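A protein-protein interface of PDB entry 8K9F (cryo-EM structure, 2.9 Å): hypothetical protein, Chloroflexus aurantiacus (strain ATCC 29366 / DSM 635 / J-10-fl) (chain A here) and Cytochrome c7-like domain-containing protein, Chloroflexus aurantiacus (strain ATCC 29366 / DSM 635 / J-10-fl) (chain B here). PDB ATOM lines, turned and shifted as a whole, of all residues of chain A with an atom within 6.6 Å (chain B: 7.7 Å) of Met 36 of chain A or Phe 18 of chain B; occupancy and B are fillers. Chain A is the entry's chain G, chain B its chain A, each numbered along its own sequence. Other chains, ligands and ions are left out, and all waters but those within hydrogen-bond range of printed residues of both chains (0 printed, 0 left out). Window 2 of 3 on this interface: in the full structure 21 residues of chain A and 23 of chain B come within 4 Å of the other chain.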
ATOM      1  N   LEU A  32      14.943  24.272  23.032  1.00  0.00           N
ATOM      2  CA  LEU A  32      15.248  25.202  21.957  1.00  0.00           C
ATOM      3  C   LEU A  32      15.503  24.463  20.661  1.00  0.00           C
ATOM      4  O   LEU A  32      15.784  23.263  20.650  1.00  0.00           O
ATOM      5  CB  LEU A  32      16.459  26.069  22.305  1.00  0.00           C
ATOM      6  CG  LEU A  32      16.194  27.499  22.782  1.00  0.00           C
ATOM      7  CD1 LEU A  32      17.386  28.039  23.545  1.00  0.00           C
ATOM      8  CD2 LEU A  32      15.861  28.395  21.600  1.00  0.00           C
ATOM      9  N   SER A  33      15.393  25.196  19.560  1.00  0.00           N
ATOM     10  CA  SER A  33      15.646  24.622  18.250  1.00  0.00           C
ATOM     11  C   SER A  33      17.058  24.885  17.768  1.00  0.00           C
ATOM     12  O   SER A  33      17.637  24.029  17.098  1.00  0.00           O
ATOM     13  CB  SER A  33      14.653  25.171  17.234  1.00  0.00           C
ATOM     14  OG  SER A  33      14.777  26.576  17.121  1.00  0.00           O
ATOM     15  N   ARG A  34      17.632  26.046  18.094  1.00  0.00           N
ATOM     16  CA  ARG A  34      19.034  26.277  17.771  1.00  0.00           C
ATOM     17  C   ARG A  34      19.946  25.348  18.564  1.00  0.00           C
ATOM     18  O   ARG A  34      21.019  24.978  18.079  1.00  0.00           O
ATOM     19  CB  ARG A  34      19.395  27.745  17.995  1.00  0.00           C
ATOM     20  CG  ARG A  34      19.404  28.209  19.445  1.00  0.00           C
ATOM     21  CD  ARG A  34      19.189  29.708  19.533  1.00  0.00           C
ATOM     22  NE  ARG A  34      17.794  30.063  19.306  1.00  0.00           N
ATOM     23  CZ  ARG A  34      17.339  30.647  18.206  1.00  0.00           C
ATOM     24  NH1 ARG A  34      18.141  30.937  17.194  1.00  0.00           N
ATOM     25  NH2 ARG A  34      16.047  30.949  18.119  1.00  0.00           N
ATOM     26  N   LEU A  35      19.509  24.909  19.750  1.00  0.00           N
ATOM     27  CA  LEU A  35      20.225  23.856  20.456  1.00  0.00           C
ATOM     28  C   LEU A  35      20.090  22.518  19.744  1.00  0.00           C
ATOM     29  O   LEU A  35      21.028  21.716  19.771  1.00  0.00           O
ATOM     30  CB  LEU A  35      19.733  23.749  21.897  1.00  0.00           C
ATOM     31  CG  LEU A  35      19.994  24.960  22.792  1.00  0.00           C
ATOM     32  CD1 LEU A  35      19.501  24.686  24.198  1.00  0.00           C
ATOM     33  CD2 LEU A  35      21.464  25.324  22.798  1.00  0.00           C
ATOM     34  N   MET A  36      18.947  22.272  19.087  1.00  0.00           N
ATOM     35  CA  MET A  36      18.796  21.060  18.282  1.00  0.00           C
ATOM     36  C   MET A  36      19.778  21.077  17.119  1.00  0.00           C
ATOM     37  O   MET A  36      20.453  20.073  16.847  1.00  0.00           O
ATOM     38  CB  MET A  36      17.363  20.926  17.767  1.00  0.00           C
ATOM     39  CG  MET A  36      16.329  20.688  18.856  1.00  0.00           C
ATOM     40  SD  MET A  36      16.640  19.180  19.792  1.00  0.00           S
ATOM     41  CE  MET A  36      16.343  17.936  18.538  1.00  0.00           C
ATOM     42  N   ILE A  37      19.881  22.230  16.434  1.00  0.00           N
ATOM     43  CA  ILE A  37      20.809  22.375  15.309  1.00  0.00           C
ATOM     44  C   ILE A  37      22.248  22.218  15.775  1.00  0.00           C
ATOM     45  O   ILE A  37      23.044  21.536  15.128  1.00  0.00           O
ATOM     46  CB  ILE A  37      20.633  23.728  14.587  1.00  0.00           C
ATOM     47  CG1 ILE A  37      19.170  24.086  14.335  1.00  0.00           C
ATOM     48  CG2 ILE A  37      21.380  23.712  13.260  1.00  0.00           C
ATOM     49  CD1 ILE A  37      18.408  23.111  13.501  1.00  0.00           C
ATOM     50  N   ALA A  38      22.603  22.844  16.900  1.00  0.00           N
ATOM     51  CA  ALA A  38      23.984  22.804  17.373  1.00  0.00           C
ATOM     52  C   ALA A  38      24.377  21.408  17.841  1.00  0.00           C
ATOM     53  O   ALA A  38      25.478  20.936  17.529  1.00  0.00           O
ATOM     54  CB  ALA A  38      24.187  23.824  18.492  1.00  0.00           C
ATOM     55  N   GLY A  39      23.485  20.726  18.564  1.00  0.00           N
ATOM     56  CA  GLY A  39      23.764  19.362  18.978  1.00  0.00           C
ATOM     57  C   GLY A  39      23.846  18.398  17.814  1.00  0.00           C
ATOM     58  O   GLY A  39      24.702  17.508  17.797  1.00  0.00           O
ATOM     59  N   LEU A  40      22.989  18.581  16.803  1.00  0.00           N
ATOM     60  CA  LEU A  40      23.059  17.700  15.644  1.00  0.00           C
ATOM     61  C   LEU A  40      24.267  18.016  14.770  1.00  0.00           C
ATOM     62  O   LEU A  40      24.845  17.112  14.170  1.00  0.00           O
ATOM     63  CB  LEU A  40      21.750  17.757  14.858  1.00  0.00           C
ATOM     64  CG  LEU A  40      21.721  16.841  13.638  1.00  0.00           C
ATOM     65  CD1 LEU A  40      20.932  15.635  13.970  1.00  0.00           C
ATOM     66  CD2 LEU A  40      21.117  17.557  12.440  1.00  0.00           C
ATOM     67  N   MET A  41      24.705  19.274  14.726  1.00  0.00           N
ATOM     68  CA  MET A  41      25.930  19.576  13.995  1.00  0.00           C
ATOM     69  C   MET A  41      27.162  19.045  14.714  1.00  0.00           C
ATOM     70  O   MET A  41      28.109  18.604  14.055  1.00  0.00           O
ATOM     71  CB  MET A  41      26.059  21.079  13.753  1.00  0.00           C
ATOM     72  CG  MET A  41      25.161  21.599  12.643  1.00  0.00           C
ATOM     73  SD  MET A  41      25.161  23.392  12.429  1.00  0.00           S
ATOM     74  CE  MET A  41      25.912  23.965  13.951  1.00  0.00           C
ATOM     75  N   LEU B  12      16.713  21.438  29.744  1.00  0.00           N
ATOM     76  CA  LEU B  12      17.614  20.323  30.006  1.00  0.00           C
ATOM     77  C   LEU B  12      16.945  18.983  29.750  1.00  0.00           C
ATOM     78  O   LEU B  12      17.607  18.049  29.294  1.00  0.00           O
ATOM     79  CB  LEU B  12      18.138  20.389  31.441  1.00  0.00           C
ATOM     80  CG  LEU B  12      19.459  21.111  31.727  1.00  0.00           C
ATOM     81  CD1 LEU B  12      19.498  22.552  31.199  1.00  0.00           C
ATOM     82  CD2 LEU B  12      19.755  21.071  33.219  1.00  0.00           C
ATOM     83  N   SER B  13      15.635  18.878  29.984  1.00  0.00           N
ATOM     84  CA  SER B  13      14.936  17.621  29.744  1.00  0.00           C
ATOM     85  C   SER B  13      14.743  17.359  28.255  1.00  0.00           C
ATOM     86  O   SER B  13      14.928  16.225  27.793  1.00  0.00           O
ATOM     87  CB  SER B  13      13.595  17.626  30.475  1.00  0.00           C
ATOM     88  OG  SER B  13      12.677  18.499  29.843  1.00  0.00           O
ATOM     89  N   ARG B  14      14.347  18.387  27.488  1.00  0.00           N
ATOM     90  CA  ARG B  14      14.249  18.229  26.036  1.00  0.00           C
ATOM     91  C   ARG B  14      15.606  17.901  25.426  1.00  0.00           C
ATOM     92  O   ARG B  14      15.720  16.988  24.593  1.00  0.00           O
ATOM     93  CB  ARG B  14      13.673  19.487  25.386  1.00  0.00           C
ATOM     94  CG  ARG B  14      12.150  19.541  25.219  1.00  0.00           C
ATOM     95  CD  ARG B  14      11.358  19.570  26.513  1.00  0.00           C
ATOM     96  NE  ARG B  14       9.942  19.801  26.258  1.00  0.00           N
ATOM     97  CZ  ARG B  14       9.123  20.430  27.089  1.00  0.00           C
ATOM     98  NH1 ARG B  14       9.532  20.853  28.271  1.00  0.00           N
ATOM     99  NH2 ARG B  14       7.861  20.635  26.728  1.00  0.00           N
ATOM    100  N   LEU B  15      16.652  18.595  25.884  1.00  0.00           N
ATOM    101  CA  LEU B  15      17.997  18.322  25.404  1.00  0.00           C
ATOM    102  C   LEU B  15      18.479  16.943  25.834  1.00  0.00           C
ATOM    103  O   LEU B  15      19.227  16.305  25.099  1.00  0.00           O
ATOM    104  CB  LEU B  15      18.960  19.397  25.909  1.00  0.00           C
ATOM    105  CG  LEU B  15      19.107  20.707  25.126  1.00  0.00           C
ATOM    106  CD1 LEU B  15      17.816  21.516  25.162  1.00  0.00           C
ATOM    107  CD2 LEU B  15      20.310  21.549  25.549  1.00  0.00           C
ATOM    108  N   SER B  16      18.022  16.448  26.987  1.00  0.00           N
ATOM    109  CA  SER B  16      18.448  15.138  27.467  1.00  0.00           C
ATOM    110  C   SER B  16      17.788  14.005  26.692  1.00  0.00           C
ATOM    111  O   SER B  16      18.450  13.013  26.372  1.00  0.00           O
ATOM    112  CB  SER B  16      18.151  15.009  28.958  1.00  0.00           C
ATOM    113  OG  SER B  16      16.812  14.607  29.174  1.00  0.00           O
ATOM    114  N   ILE B  17      16.487  14.120  26.397  1.00  0.00           N
ATOM    115  CA  ILE B  17      15.825  13.117  25.557  1.00  0.00           C
ATOM    116  C   ILE B  17      16.419  13.117  24.150  1.00  0.00           C
ATOM    117  O   ILE B  17      16.689  12.046  23.570  1.00  0.00           O
ATOM    118  CB  ILE B  17      14.299  13.343  25.528  1.00  0.00           C
ATOM    119  CG1 ILE B  17      13.709  13.328  26.944  1.00  0.00           C
ATOM    120  CG2 ILE B  17      13.608  12.308  24.652  1.00  0.00           C
ATOM    121  CD1 ILE B  17      13.651  11.961  27.587  1.00  0.00           C
ATOM    122  N   PHE B  18      16.674  14.316  23.599  1.00  0.00           N
ATOM    123  CA  PHE B  18      17.318  14.413  22.290  1.00  0.00           C
ATOM    124  C   PHE B  18      18.724  13.830  22.309  1.00  0.00           C
ATOM    125  O   PHE B  18      19.125  13.131  21.370  1.00  0.00           O
ATOM    126  CB  PHE B  18      17.411  15.863  21.840  1.00  0.00           C
ATOM    127  CG  PHE B  18      17.885  16.000  20.437  1.00  0.00           C
ATOM    128  CD1 PHE B  18      17.326  15.216  19.446  1.00  0.00           C
ATOM    129  CD2 PHE B  18      18.968  16.806  20.120  1.00  0.00           C
ATOM    130  CE1 PHE B  18      17.765  15.311  18.151  1.00  0.00           C
ATOM    131  CE2 PHE B  18      19.411  16.907  18.821  1.00  0.00           C
ATOM    132  CZ  PHE B  18      18.813  16.151  17.834  1.00  0.00           C
ATOM    133  N   ALA B  19      19.481  14.114  23.368  1.00  0.00           N
ATOM    134  CA  ALA B  19      20.838  13.612  23.492  1.00  0.00           C
ATOM    135  C   ALA B  19      20.862  12.107  23.664  1.00  0.00           C
ATOM    136  O   ALA B  19      21.773  11.462  23.157  1.00  0.00           O
ATOM    137  CB  ALA B  19      21.547  14.290  24.664  1.00  0.00           C
ATOM    138  N   LEU B  20      19.883  11.535  24.372  1.00  0.00           N
ATOM    139  CA  LEU B  20      19.805  10.082  24.493  1.00  0.00           C
ATOM    140  C   LEU B  20      19.568   9.428  23.140  1.00  0.00           C
ATOM    141  O   LEU B  20      20.216   8.423  22.811  1.00  0.00           O
ATOM    142  CB  LEU B  20      18.705   9.692  25.476  1.00  0.00           C
ATOM    143  CG  LEU B  20      18.570   8.187  25.721  1.00  0.00           C
ATOM    144  CD1 LEU B  20      19.117   7.795  27.089  1.00  0.00           C
ATOM    145  CD2 LEU B  20      17.125   7.754  25.572  1.00  0.00           C
ATOM    146  N   VAL B  21      18.669  10.012  22.330  1.00  0.00           N
ATOM    147  CA  VAL B  21      18.453   9.512  20.969  1.00  0.00           C
ATOM    148  C   VAL B  21      19.735   9.620  20.144  1.00  0.00           C
ATOM    149  O   VAL B  21      20.134   8.667  19.454  1.00  0.00           O
ATOM    150  CB  VAL B  21      17.279  10.257  20.305  1.00  0.00           C
ATOM    151  CG1 VAL B  21      17.278  10.060  18.798  1.00  0.00           C
ATOM    152  CG2 VAL B  21      15.960   9.788  20.887  1.00  0.00           C
ATOM    153  N   LEU B  22      20.437  10.752  20.264  1.00  0.00           N
ATOM    154  CA  LEU B  22      21.655  10.964  19.487  1.00  0.00           C
ATOM    155  C   LEU B  22      22.808  10.069  19.936  1.00  0.00           C
ATOM    156  O   LEU B  22      23.590   9.632  19.094  1.00  0.00           O
ATOM    157  CB  LEU B  22      22.069  12.432  19.541  1.00  0.00           C
ATOM    158  CG  LEU B  22      21.381  13.398  18.570  1.00  0.00           C
ATOM    159  CD1 LEU B  22      22.220  14.654  18.410  1.00  0.00           C
ATOM    160  CD2 LEU B  22      21.121  12.760  17.216  1.00  0.00           C
ATOM    161  N   LEU B  23      22.942   9.777  21.235  1.00  0.00           N
ATOM    162  CA  LEU B  23      23.990   8.843  21.652  1.00  0.00           C
ATOM    163  C   LEU B  23      23.654   7.403  21.303  1.00  0.00           C
ATOM    164  O   LEU B  23      24.572   6.611  21.088  1.00  0.00           O
ATOM    165  CB  LEU B  23      24.312   8.925  23.149  1.00  0.00           C
ATOM    166  CG  LEU B  23      24.578  10.196  23.951  1.00  0.00           C
ATOM    167  CD1 LEU B  23      24.539   9.888  25.444  1.00  0.00           C
ATOM    168  CD2 LEU B  23      25.907  10.825  23.558  1.00  0.00           C
ATOM    169  N   VAL B  24      22.369   7.038  21.243  1.00  0.00           N
ATOM    170  CA  VAL B  24      22.018   5.719  20.714  1.00  0.00           C
ATOM    171  C   VAL B  24      22.412   5.608  19.242  1.00  0.00           C
ATOM    172  O   VAL B  24      23.057   4.629  18.828  1.00  0.00           O
ATOM    173  CB  VAL B  24      20.518   5.443  20.931  1.00  0.00           C
ATOM    174  CG1 VAL B  24      20.042   4.283  20.069  1.00  0.00           C
ATOM    175  CG2 VAL B  24      20.248   5.146  22.396  1.00  0.00           C
ATOM    176  N   VAL B  25      22.079   6.637  18.451  1.00  0.00           N
ATOM    177  CA  VAL B  25      22.441   6.680  17.033  1.00  0.00           C
ATOM    178  C   VAL B  25      23.958   6.681  16.863  1.00  0.00           C
ATOM    179  O   VAL B  25      24.509   5.967  16.011  1.00  0.00           O
ATOM    180  CB  VAL B  25      21.785   7.908  16.369  1.00  0.00           C
ATOM    181  CG1 VAL B  25      22.373   8.191  14.996  1.00  0.00           C
ATOM    182  CG2 VAL B  25      20.275   7.719  16.269  1.00  0.00           C
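Of the printed residues of chain B, Leu 35 of chain A touches Leu 15 (3.5 Å).
Of chain B, only Phe 18 (3.0 Å) comes within 4 Å of Met 36 of chain A.
Printed residues of chain B within 4 Å of Gly 39 of chain A: Leu 22.
Of the printed residues of chain A, Leu 15 of chain B touches Leu 35 (3.5 Å).
Phe 18 of chain B touches one residue of chain A.
Printed residues of chain A within 4 Å of Leu 22 of chain B: Gly 39.
Leu 23 of chain B touches none of the printed residues of chain A.
Val 25 of chain B touches none of the printed residues of chain A.
The nearest printed residue of chain B that does not touch Leu 35 of chain A is Phe 18 of chain B (5.2 Å).
Among the printed residues, pairs that only touch across the chains: Leu 35 of chain A with Leu 15 of chain B, Met 36 of chain A with Phe 18 of chain B and Gly 39 of chain A with Leu 22 of chain B.
Printed residues of chain A that touch a printed residue of chain B: Leu 35, Met 36 and Gly 39.
Hydrophobic or aromatic side chains of chain A within 4 Å of the printed part of chain B: Leu 35 and Met 36.
Of the 14 printed residues of chain B, 3 touch a printed residue of chain A.
Among the printed residues, 3 pairs touch across the chains.
Among the printed residues, no Asp or Glu carboxylate lies within 4 Å of a Lys or Arg side-chain nitrogen of the other chain.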
